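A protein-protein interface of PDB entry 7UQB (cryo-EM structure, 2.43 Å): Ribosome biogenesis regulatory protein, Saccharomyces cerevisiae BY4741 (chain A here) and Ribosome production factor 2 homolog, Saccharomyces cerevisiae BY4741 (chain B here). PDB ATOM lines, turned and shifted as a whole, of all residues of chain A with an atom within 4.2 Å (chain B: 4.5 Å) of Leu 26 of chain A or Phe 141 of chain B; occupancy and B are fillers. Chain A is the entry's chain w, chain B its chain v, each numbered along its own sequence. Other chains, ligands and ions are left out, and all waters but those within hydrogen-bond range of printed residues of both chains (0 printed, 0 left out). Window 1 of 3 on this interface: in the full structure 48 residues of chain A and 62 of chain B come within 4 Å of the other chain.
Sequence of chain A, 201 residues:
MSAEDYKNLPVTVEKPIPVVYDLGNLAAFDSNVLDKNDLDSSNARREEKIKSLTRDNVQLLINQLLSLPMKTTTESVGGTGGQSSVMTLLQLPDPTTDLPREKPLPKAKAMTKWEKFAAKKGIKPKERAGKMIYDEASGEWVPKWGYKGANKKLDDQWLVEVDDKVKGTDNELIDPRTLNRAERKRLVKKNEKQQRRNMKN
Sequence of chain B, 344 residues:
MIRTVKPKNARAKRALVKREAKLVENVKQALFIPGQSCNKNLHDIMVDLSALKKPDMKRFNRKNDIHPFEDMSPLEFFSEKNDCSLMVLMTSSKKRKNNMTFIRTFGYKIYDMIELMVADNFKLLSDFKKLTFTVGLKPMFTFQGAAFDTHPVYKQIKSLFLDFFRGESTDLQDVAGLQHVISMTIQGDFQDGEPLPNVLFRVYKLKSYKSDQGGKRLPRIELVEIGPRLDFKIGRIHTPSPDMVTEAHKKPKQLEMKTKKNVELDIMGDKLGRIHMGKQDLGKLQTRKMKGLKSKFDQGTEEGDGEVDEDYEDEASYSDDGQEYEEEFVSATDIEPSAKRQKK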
ATOM      1  N   ASP A  22       9.486  14.355  -3.869  1.00  0.00           N
ATOM      2  CA  ASP A  22       8.203  14.691  -3.260  1.00  0.00           C
ATOM      3  C   ASP A  22       8.438  14.544  -1.760  1.00  0.00           C
ATOM      4  O   ASP A  22       8.220  13.471  -1.190  1.00  0.00           O
ATOM      5  CB  ASP A  22       7.085  13.784  -3.765  1.00  0.00           C
ATOM      6  CG  ASP A  22       5.718  14.218  -3.280  1.00  0.00           C
ATOM      7  OD1 ASP A  22       5.608  15.320  -2.705  1.00  0.00           O
ATOM      8  OD2 ASP A  22       4.750  13.455  -3.474  1.00  0.00           O
ATOM      9  N   LEU A  23       8.921  15.616  -1.130  1.00  0.00           N
ATOM     10  CA  LEU A  23       9.279  15.549   0.281  1.00  0.00           C
ATOM     11  C   LEU A  23       8.060  15.449   1.186  1.00  0.00           C
ATOM     12  O   LEU A  23       8.177  14.938   2.305  1.00  0.00           O
ATOM     13  CB  LEU A  23      10.123  16.765   0.662  1.00  0.00           C
ATOM     14  CG  LEU A  23      11.427  16.929  -0.118  1.00  0.00           C
ATOM     15  CD1 LEU A  23      12.118  18.223   0.261  1.00  0.00           C
ATOM     16  CD2 LEU A  23      12.351  15.740   0.110  1.00  0.00           C
ATOM     17  N   GLY A  24       6.899  15.924   0.732  1.00  0.00           N
ATOM     18  CA  GLY A  24       5.685  15.749   1.512  1.00  0.00           C
ATOM     19  C   GLY A  24       5.291  14.291   1.650  1.00  0.00           C
ATOM     20  O   GLY A  24       4.739  13.882   2.674  1.00  0.00           O
ATOM     21  N   ASN A  25       5.562  13.492   0.620  1.00  0.00           N
ATOM     22  CA  ASN A  25       5.315  12.058   0.646  1.00  0.00           C
ATOM     23  C   ASN A  25       6.557  11.247   0.987  1.00  0.00           C
ATOM     24  O   ASN A  25       6.480  10.014   1.008  1.00  0.00           O
ATOM     25  CB  ASN A  25       4.755  11.592  -0.702  1.00  0.00           C
ATOM     26  CG  ASN A  25       3.342  12.080  -0.945  1.00  0.00           C
ATOM     27  OD1 ASN A  25       2.549  12.206  -0.015  1.00  0.00           O
ATOM     28  ND2 ASN A  25       3.020  12.357  -2.202  1.00  0.00           N
ATOM     29  N   LEU A  26       7.687  11.909   1.255  1.00  0.00           N
ATOM     30  CA  LEU A  26       8.969  11.254   1.540  1.00  0.00           C
ATOM     31  C   LEU A  26       9.376  10.306   0.410  1.00  0.00           C
ATOM     32  O   LEU A  26       9.803   9.174   0.643  1.00  0.00           O
ATOM     33  CB  LEU A  26       8.928  10.514   2.882  1.00  0.00           C
ATOM     34  CG  LEU A  26       8.654  11.312   4.156  1.00  0.00           C
ATOM     35  CD1 LEU A  26       8.528  10.378   5.346  1.00  0.00           C
ATOM     36  CD2 LEU A  26       9.754  12.323   4.391  1.00  0.00           C
ATOM     37  N   ALA A  27       9.243  10.779  -0.828  1.00  0.00           N
ATOM     38  CA  ALA A  27       9.463   9.945  -2.000  1.00  0.00           C
ATOM     39  C   ALA A  27      10.464  10.594  -2.945  1.00  0.00           C
ATOM     40  O   ALA A  27      10.562  11.820  -3.033  1.00  0.00           O
ATOM     41  CB  ALA A  27       8.149   9.680  -2.746  1.00  0.00           C
ATOM     42  N   ALA A  28      11.207   9.750  -3.656  1.00  0.00           N
ATOM     43  CA  ALA A  28      12.122  10.188  -4.698  1.00  0.00           C
ATOM     44  C   ALA A  28      11.823   9.415  -5.974  1.00  0.00           C
ATOM     45  O   ALA A  28      11.405   8.255  -5.929  1.00  0.00           O
ATOM     46  CB  ALA A  28      13.585   9.984  -4.289  1.00  0.00           C
ATOM     47  N   LEU A  61      17.588  11.429  -1.033  1.00  0.00           N
ATOM     48  CA  LEU A  61      16.376  11.838  -0.330  1.00  0.00           C
ATOM     49  C   LEU A  61      16.680  12.297   1.092  1.00  0.00           C
ATOM     50  O   LEU A  61      16.118  13.292   1.562  1.00  0.00           O
ATOM     51  CB  LEU A  61      15.367  10.690  -0.319  1.00  0.00           C
ATOM     52  CG  LEU A  61      14.027  10.961   0.364  1.00  0.00           C
ATOM     53  CD1 LEU A  61      13.265  12.061  -0.355  1.00  0.00           C
ATOM     54  CD2 LEU A  61      13.201   9.689   0.435  1.00  0.00           C
ATOM     55  N   LEU A  65      16.029  15.865   2.871  1.00  0.00           N
ATOM     56  CA  LEU A  65      15.254  15.969   4.105  1.00  0.00           C
ATOM     57  C   LEU A  65      16.039  16.682   5.199  1.00  0.00           C
ATOM     58  O   LEU A  65      15.475  17.483   5.953  1.00  0.00           O
ATOM     59  CB  LEU A  65      14.825  14.581   4.577  1.00  0.00           C
ATOM     60  CG  LEU A  65      13.754  13.888   3.738  1.00  0.00           C
ATOM     61  CD1 LEU A  65      13.504  12.477   4.244  1.00  0.00           C
ATOM     62  CD2 LEU A  65      12.475  14.703   3.746  1.00  0.00           C
ATOM     63  N   LYS B 138       5.216   6.081   8.950  1.00  0.00           N
ATOM     64  CA  LYS B 138       5.189   6.178   7.499  1.00  0.00           C
ATOM     65  C   LYS B 138       6.587   5.962   6.922  1.00  0.00           C
ATOM     66  O   LYS B 138       7.578   6.436   7.487  1.00  0.00           O
ATOM     67  CB  LYS B 138       4.624   7.528   7.050  1.00  0.00           C
ATOM     68  CG  LYS B 138       5.395   8.754   7.501  1.00  0.00           C
ATOM     69  CD  LYS B 138       4.771  10.016   6.922  1.00  0.00           C
ATOM     70  CE  LYS B 138       4.628   9.913   5.411  1.00  0.00           C
ATOM     71  NZ  LYS B 138       3.812  11.020   4.839  1.00  0.00           N
ATOM     72  N   PRO B 139       6.702   5.238   5.815  1.00  0.00           N
ATOM     73  CA  PRO B 139       8.011   4.925   5.245  1.00  0.00           C
ATOM     74  C   PRO B 139       8.490   5.987   4.264  1.00  0.00           C
ATOM     75  O   PRO B 139       7.754   6.893   3.869  1.00  0.00           O
ATOM     76  CB  PRO B 139       7.747   3.608   4.508  1.00  0.00           C
ATOM     77  CG  PRO B 139       6.337   3.749   4.042  1.00  0.00           C
ATOM     78  CD  PRO B 139       5.617   4.517   5.126  1.00  0.00           C
ATOM     79  N   MET B 140       9.750   5.852   3.872  1.00  0.00           N
ATOM     80  CA  MET B 140      10.248   6.558   2.705  1.00  0.00           C
ATOM     81  C   MET B 140       9.958   5.731   1.457  1.00  0.00           C
ATOM     82  O   MET B 140       9.692   4.532   1.533  1.00  0.00           O
ATOM     83  CB  MET B 140      11.744   6.838   2.839  1.00  0.00           C
ATOM     84  CG  MET B 140      12.071   7.946   3.826  1.00  0.00           C
ATOM     85  SD  MET B 140      13.746   7.852   4.479  1.00  0.00           S
ATOM     86  CE  MET B 140      13.592   6.445   5.574  1.00  0.00           C
ATOM     87  N   PHE B 141       9.992   6.386   0.301  1.00  0.00           N
ATOM     88  CA  PHE B 141       9.673   5.728  -0.957  1.00  0.00           C
ATOM     89  C   PHE B 141      10.746   6.013  -1.993  1.00  0.00           C
ATOM     90  O   PHE B 141      11.237   7.141  -2.098  1.00  0.00           O
ATOM     91  CB  PHE B 141       8.318   6.185  -1.506  1.00  0.00           C
ATOM     92  CG  PHE B 141       7.150   5.764  -0.668  1.00  0.00           C
ATOM     93  CD1 PHE B 141       6.646   4.479  -0.757  1.00  0.00           C
ATOM     94  CD2 PHE B 141       6.545   6.659   0.196  1.00  0.00           C
ATOM     95  CE1 PHE B 141       5.569   4.091   0.010  1.00  0.00           C
ATOM     96  CE2 PHE B 141       5.469   6.279   0.964  1.00  0.00           C
ATOM     97  CZ  PHE B 141       4.979   4.995   0.871  1.00  0.00           C
ATOM     98  N   THR B 142      11.108   4.984  -2.757  1.00  0.00           N
ATOM     99  CA  THR B 142      11.927   5.155  -3.950  1.00  0.00           C
ATOM    100  C   THR B 142      11.269   4.415  -5.105  1.00  0.00           C
ATOM    101  O   THR B 142      10.845   3.266  -4.948  1.00  0.00           O
ATOM    102  CB  THR B 142      13.362   4.649  -3.749  1.00  0.00           C
ATOM    103  OG1 THR B 142      13.337   3.270  -3.372  1.00  0.00           O
ATOM    104  CG2 THR B 142      14.078   5.455  -2.673  1.00  0.00           C
ATOM    105  N   PHE B 143      11.162   5.085  -6.249  1.00  0.00           N
ATOM    106  CA  PHE B 143      10.616   4.502  -7.469  1.00  0.00           C
ATOM    107  C   PHE B 143      11.670   4.596  -8.561  1.00  0.00           C
ATOM    108  O   PHE B 143      12.100   5.698  -8.918  1.00  0.00           O
ATOM    109  CB  PHE B 143       9.329   5.211  -7.894  1.00  0.00           C
ATOM    110  CG  PHE B 143       8.147   4.901  -7.019  1.00  0.00           C
ATOM    111  CD1 PHE B 143       7.337   3.813  -7.290  1.00  0.00           C
ATOM    112  CD2 PHE B 143       7.848   5.697  -5.927  1.00  0.00           C
ATOM    113  CE1 PHE B 143       6.248   3.523  -6.489  1.00  0.00           C
ATOM    114  CE2 PHE B 143       6.759   5.415  -5.123  1.00  0.00           C
ATOM    115  CZ  PHE B 143       5.958   4.327  -5.404  1.00  0.00           C
ATOM    116  N   PHE B 161       0.560   2.522  -4.987  1.00  0.00           N
ATOM    117  CA  PHE B 161       1.383   2.115  -3.854  1.00  0.00           C
ATOM    118  C   PHE B 161       1.726   3.292  -2.949  1.00  0.00           C
ATOM    119  O   PHE B 161       1.813   3.118  -1.725  1.00  0.00           O
ATOM    120  CB  PHE B 161       2.640   1.400  -4.346  1.00  0.00           C
ATOM    121  CG  PHE B 161       2.411  -0.054  -4.657  1.00  0.00           C
ATOM    122  CD1 PHE B 161       1.778  -0.434  -5.829  1.00  0.00           C
ATOM    123  CD2 PHE B 161       2.806  -1.038  -3.767  1.00  0.00           C
ATOM    124  CE1 PHE B 161       1.557  -1.768  -6.114  1.00  0.00           C
ATOM    125  CE2 PHE B 161       2.589  -2.374  -4.046  1.00  0.00           C
ATOM    126  CZ  PHE B 161       1.962  -2.739  -5.220  1.00  0.00           C
ATOM    127  N   LEU B 162       1.890   4.494  -3.516  1.00  0.00           N
ATOM    128  CA  LEU B 162       2.030   5.681  -2.678  1.00  0.00           C
ATOM    129  C   LEU B 162       0.786   5.899  -1.827  1.00  0.00           C
ATOM    130  O   LEU B 162       0.888   6.182  -0.629  1.00  0.00           O
ATOM    131  CB  LEU B 162       2.307   6.909  -3.544  1.00  0.00           C
ATOM    132  CG  LEU B 162       3.770   7.201  -3.865  1.00  0.00           C
ATOM    133  CD1 LEU B 162       3.875   8.207  -4.998  1.00  0.00           C
ATOM    134  CD2 LEU B 162       4.480   7.714  -2.624  1.00  0.00           C
ATOM    135  N   PHE B 165       0.667   2.952   1.001  1.00  0.00           N
ATOM    136  CA  PHE B 165       1.624   2.978   2.099  1.00  0.00           C
ATOM    137  C   PHE B 165       1.930   4.386   2.594  1.00  0.00           C
ATOM    138  O   PHE B 165       2.853   4.557   3.396  1.00  0.00           O
ATOM    139  CB  PHE B 165       2.915   2.272   1.685  1.00  0.00           C
ATOM    140  CG  PHE B 165       2.731   0.819   1.364  1.00  0.00           C
ATOM    141  CD1 PHE B 165       2.618  -0.117   2.378  1.00  0.00           C
ATOM    142  CD2 PHE B 165       2.667   0.388   0.050  1.00  0.00           C
ATOM    143  CE1 PHE B 165       2.445  -1.458   2.088  1.00  0.00           C
ATOM    144  CE2 PHE B 165       2.495  -0.952  -0.246  1.00  0.00           C
ATOM    145  CZ  PHE B 165       2.384  -1.875   0.775  1.00  0.00           C
ATOM    146  N   ARG B 166       1.182   5.394   2.140  1.00  0.00           N
ATOM    147  CA  ARG B 166       1.448   6.762   2.573  1.00  0.00           C
ATOM    148  C   ARG B 166       1.182   6.941   4.063  1.00  0.00           C
ATOM    149  O   ARG B 166       1.974   7.575   4.769  1.00  0.00           O
ATOM    150  CB  ARG B 166       0.608   7.740   1.753  1.00  0.00           C
ATOM    151  CG  ARG B 166       0.931   9.195   2.021  1.00  0.00           C
ATOM    152  CD  ARG B 166       0.241  10.117   1.032  1.00  0.00           C
ATOM    153  NE  ARG B 166      -1.199   9.904   0.984  1.00  0.00           N
ATOM    154  CZ  ARG B 166      -2.073  10.812   0.572  1.00  0.00           C
ATOM    155  NH1 ARG B 166      -1.689  12.025   0.206  1.00  0.00           N
ATOM    156  NH2 ARG B 166      -3.365  10.499   0.532  1.00  0.00           N
ATOM    157  N   LEU B 178      12.634   8.218  10.710  1.00  0.00           N
ATOM    158  CA  LEU B 178      13.055   7.857   9.355  1.00  0.00           C
ATOM    159  C   LEU B 178      13.764   6.509   9.429  1.00  0.00           C
ATOM    160  O   LEU B 178      14.993   6.406   9.440  1.00  0.00           O
ATOM    161  CB  LEU B 178      13.946   8.937   8.757  1.00  0.00           C
ATOM    162  CG  LEU B 178      13.296  10.306   8.563  1.00  0.00           C
ATOM    163  CD1 LEU B 178      14.290  11.285   7.970  1.00  0.00           C
ATOM    164  CD2 LEU B 178      12.057  10.193   7.689  1.00  0.00           C
ATOM    165  N   VAL B 181      12.553   2.254   4.166  1.00  0.00           N
ATOM    166  CA  VAL B 181      12.212   2.703   2.824  1.00  0.00           C
ATOM    167  C   VAL B 181      11.624   1.533   2.045  1.00  0.00           C
ATOM    168  O   VAL B 181      12.125   0.403   2.115  1.00  0.00           O
ATOM    169  CB  VAL B 181      13.438   3.298   2.096  1.00  0.00           C
ATOM    170  CG1 VAL B 181      14.628   2.350   2.171  1.00  0.00           C
ATOM    171  CG2 VAL B 181      13.102   3.637   0.650  1.00  0.00           C
ATOM    172  N   ILE B 182      10.532   1.802   1.335  1.00  0.00           N
ATOM    173  CA  ILE B 182       9.960   0.892   0.355  1.00  0.00           C
ATOM    174  C   ILE B 182      10.496   1.279  -1.017  1.00  0.00           C
ATOM    175  O   ILE B 182      10.418   2.449  -1.419  1.00  0.00           O
ATOM    176  CB  ILE B 182       8.423   0.942   0.384  1.00  0.00           C
ATOM    177  CG1 ILE B 182       7.895   0.356   1.694  1.00  0.00           C
ATOM    178  CG2 ILE B 182       7.837   0.217  -0.815  1.00  0.00           C
ATOM    179  CD1 ILE B 182       6.396   0.462   1.846  1.00  0.00           C
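Gly 24 of chain A touches Lys 138 of chain B (O to NZ, 3.7 Å). Asn 25 of chain A touches Phe 141 of chain B (O to CD2, 3.5 Å). Arg 166 of chain B touches Asn 25 of chain A. Lys 138 of chain B touches Leu 26 of chain A. Leu 26 of chain A touches Pro 139 of chain B. O of Leu 26 of chain A touches CA of Met 140 of chain B, 3.4 Å away. Phe 141 of chain B touches Ala 27 of chain A. Thr 142 of chain B touches Ala 28 of chain A. Met 140 of chain B touches Leu 61 of chain A (CG to CD2, 3.98 Å). Leu 178 of chain B touches Leu 65 of chain A (CD1 to CD1, 3.99 Å).
Of the 9 printed residues of chain A, 7 touch a printed residue of chain B. Printed residues of chain A that touch a printed residue of chain B: Gly 24, Asn 25, Leu 26, Ala 27, Ala 28, Leu 61 and Leu 65. Hydrophobic or aromatic side chains of chain A that line the printed part of chain B: Leu 26, Ala 27, Leu 61 and Leu 65. Of the 13 printed residues of chain B, 8 touch a printed residue of chain A. Hydrophobic or aromatic side chains of chain B that line the printed part of chain A: Met 140, Phe 141 and Leu 178. Among the printed residues, 13 pairs touch across the chains.
N of Phe 141 of chain B is in hydrogen-bond range of O of Leu 26 of chain A (2.8 Å). The backbone NH of Ala 28 of chain A is in hydrogen-bond range of the backbone carbonyl oxygen of Phe 141 of chain B (3.0 Å). N of Phe 143 of chain B is in hydrogen-bond range of O of Ala 28 of chain A.
The backbone carbonyl oxygen (O) of Met 140 of chain B sits at hydrogen-bond distance from the backbone NH (N) of Ile 182 of chain B, 2.9 Å away. N of Thr 142 of chain B is in hydrogen-bond range of O of Ile 182 of chain B (2.9 Å). The side-chain carboxylate (OD2) of Asp 22 of chain A lies within hydrogen-bond range of the side-chain amide nitrogen (ND2) of Asn 25 of chain A (2.4 Å). N of Asp 22 of chain A lies within hydrogen-bond range of O of Ala 27 of chain A, 2.9 Å away.
Of chain B, only Lys 138 (3.9 Å), Pro 139 (3.9 Å), Met 140 (3.4 Å) and Phe 141 (2.8 Å) come within 4 Å of Leu 26 of chain A. Of the printed residues of chain A, Phe 141 of chain B touches Asn 25, Leu 26, Ala 27 and Ala 28. Of the printed residues of chain A, Lys 138 of chain B touches Gly 24 and Leu 26. Of the printed residues of chain B, Leu 65 of chain A touches Leu 178. Printed residues of chain B within 4 Å of Asn 25 of chain A: Phe 141 and Arg 166. Of the printed residues of chain B, Leu 61 of chain A touches Met 140. Ile 182 of chain B touches none of the printed residues of chain A. The nearest residue of chain A that does not touch Phe 141 of chain B is Leu 61 of chain A (4.1 Å).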
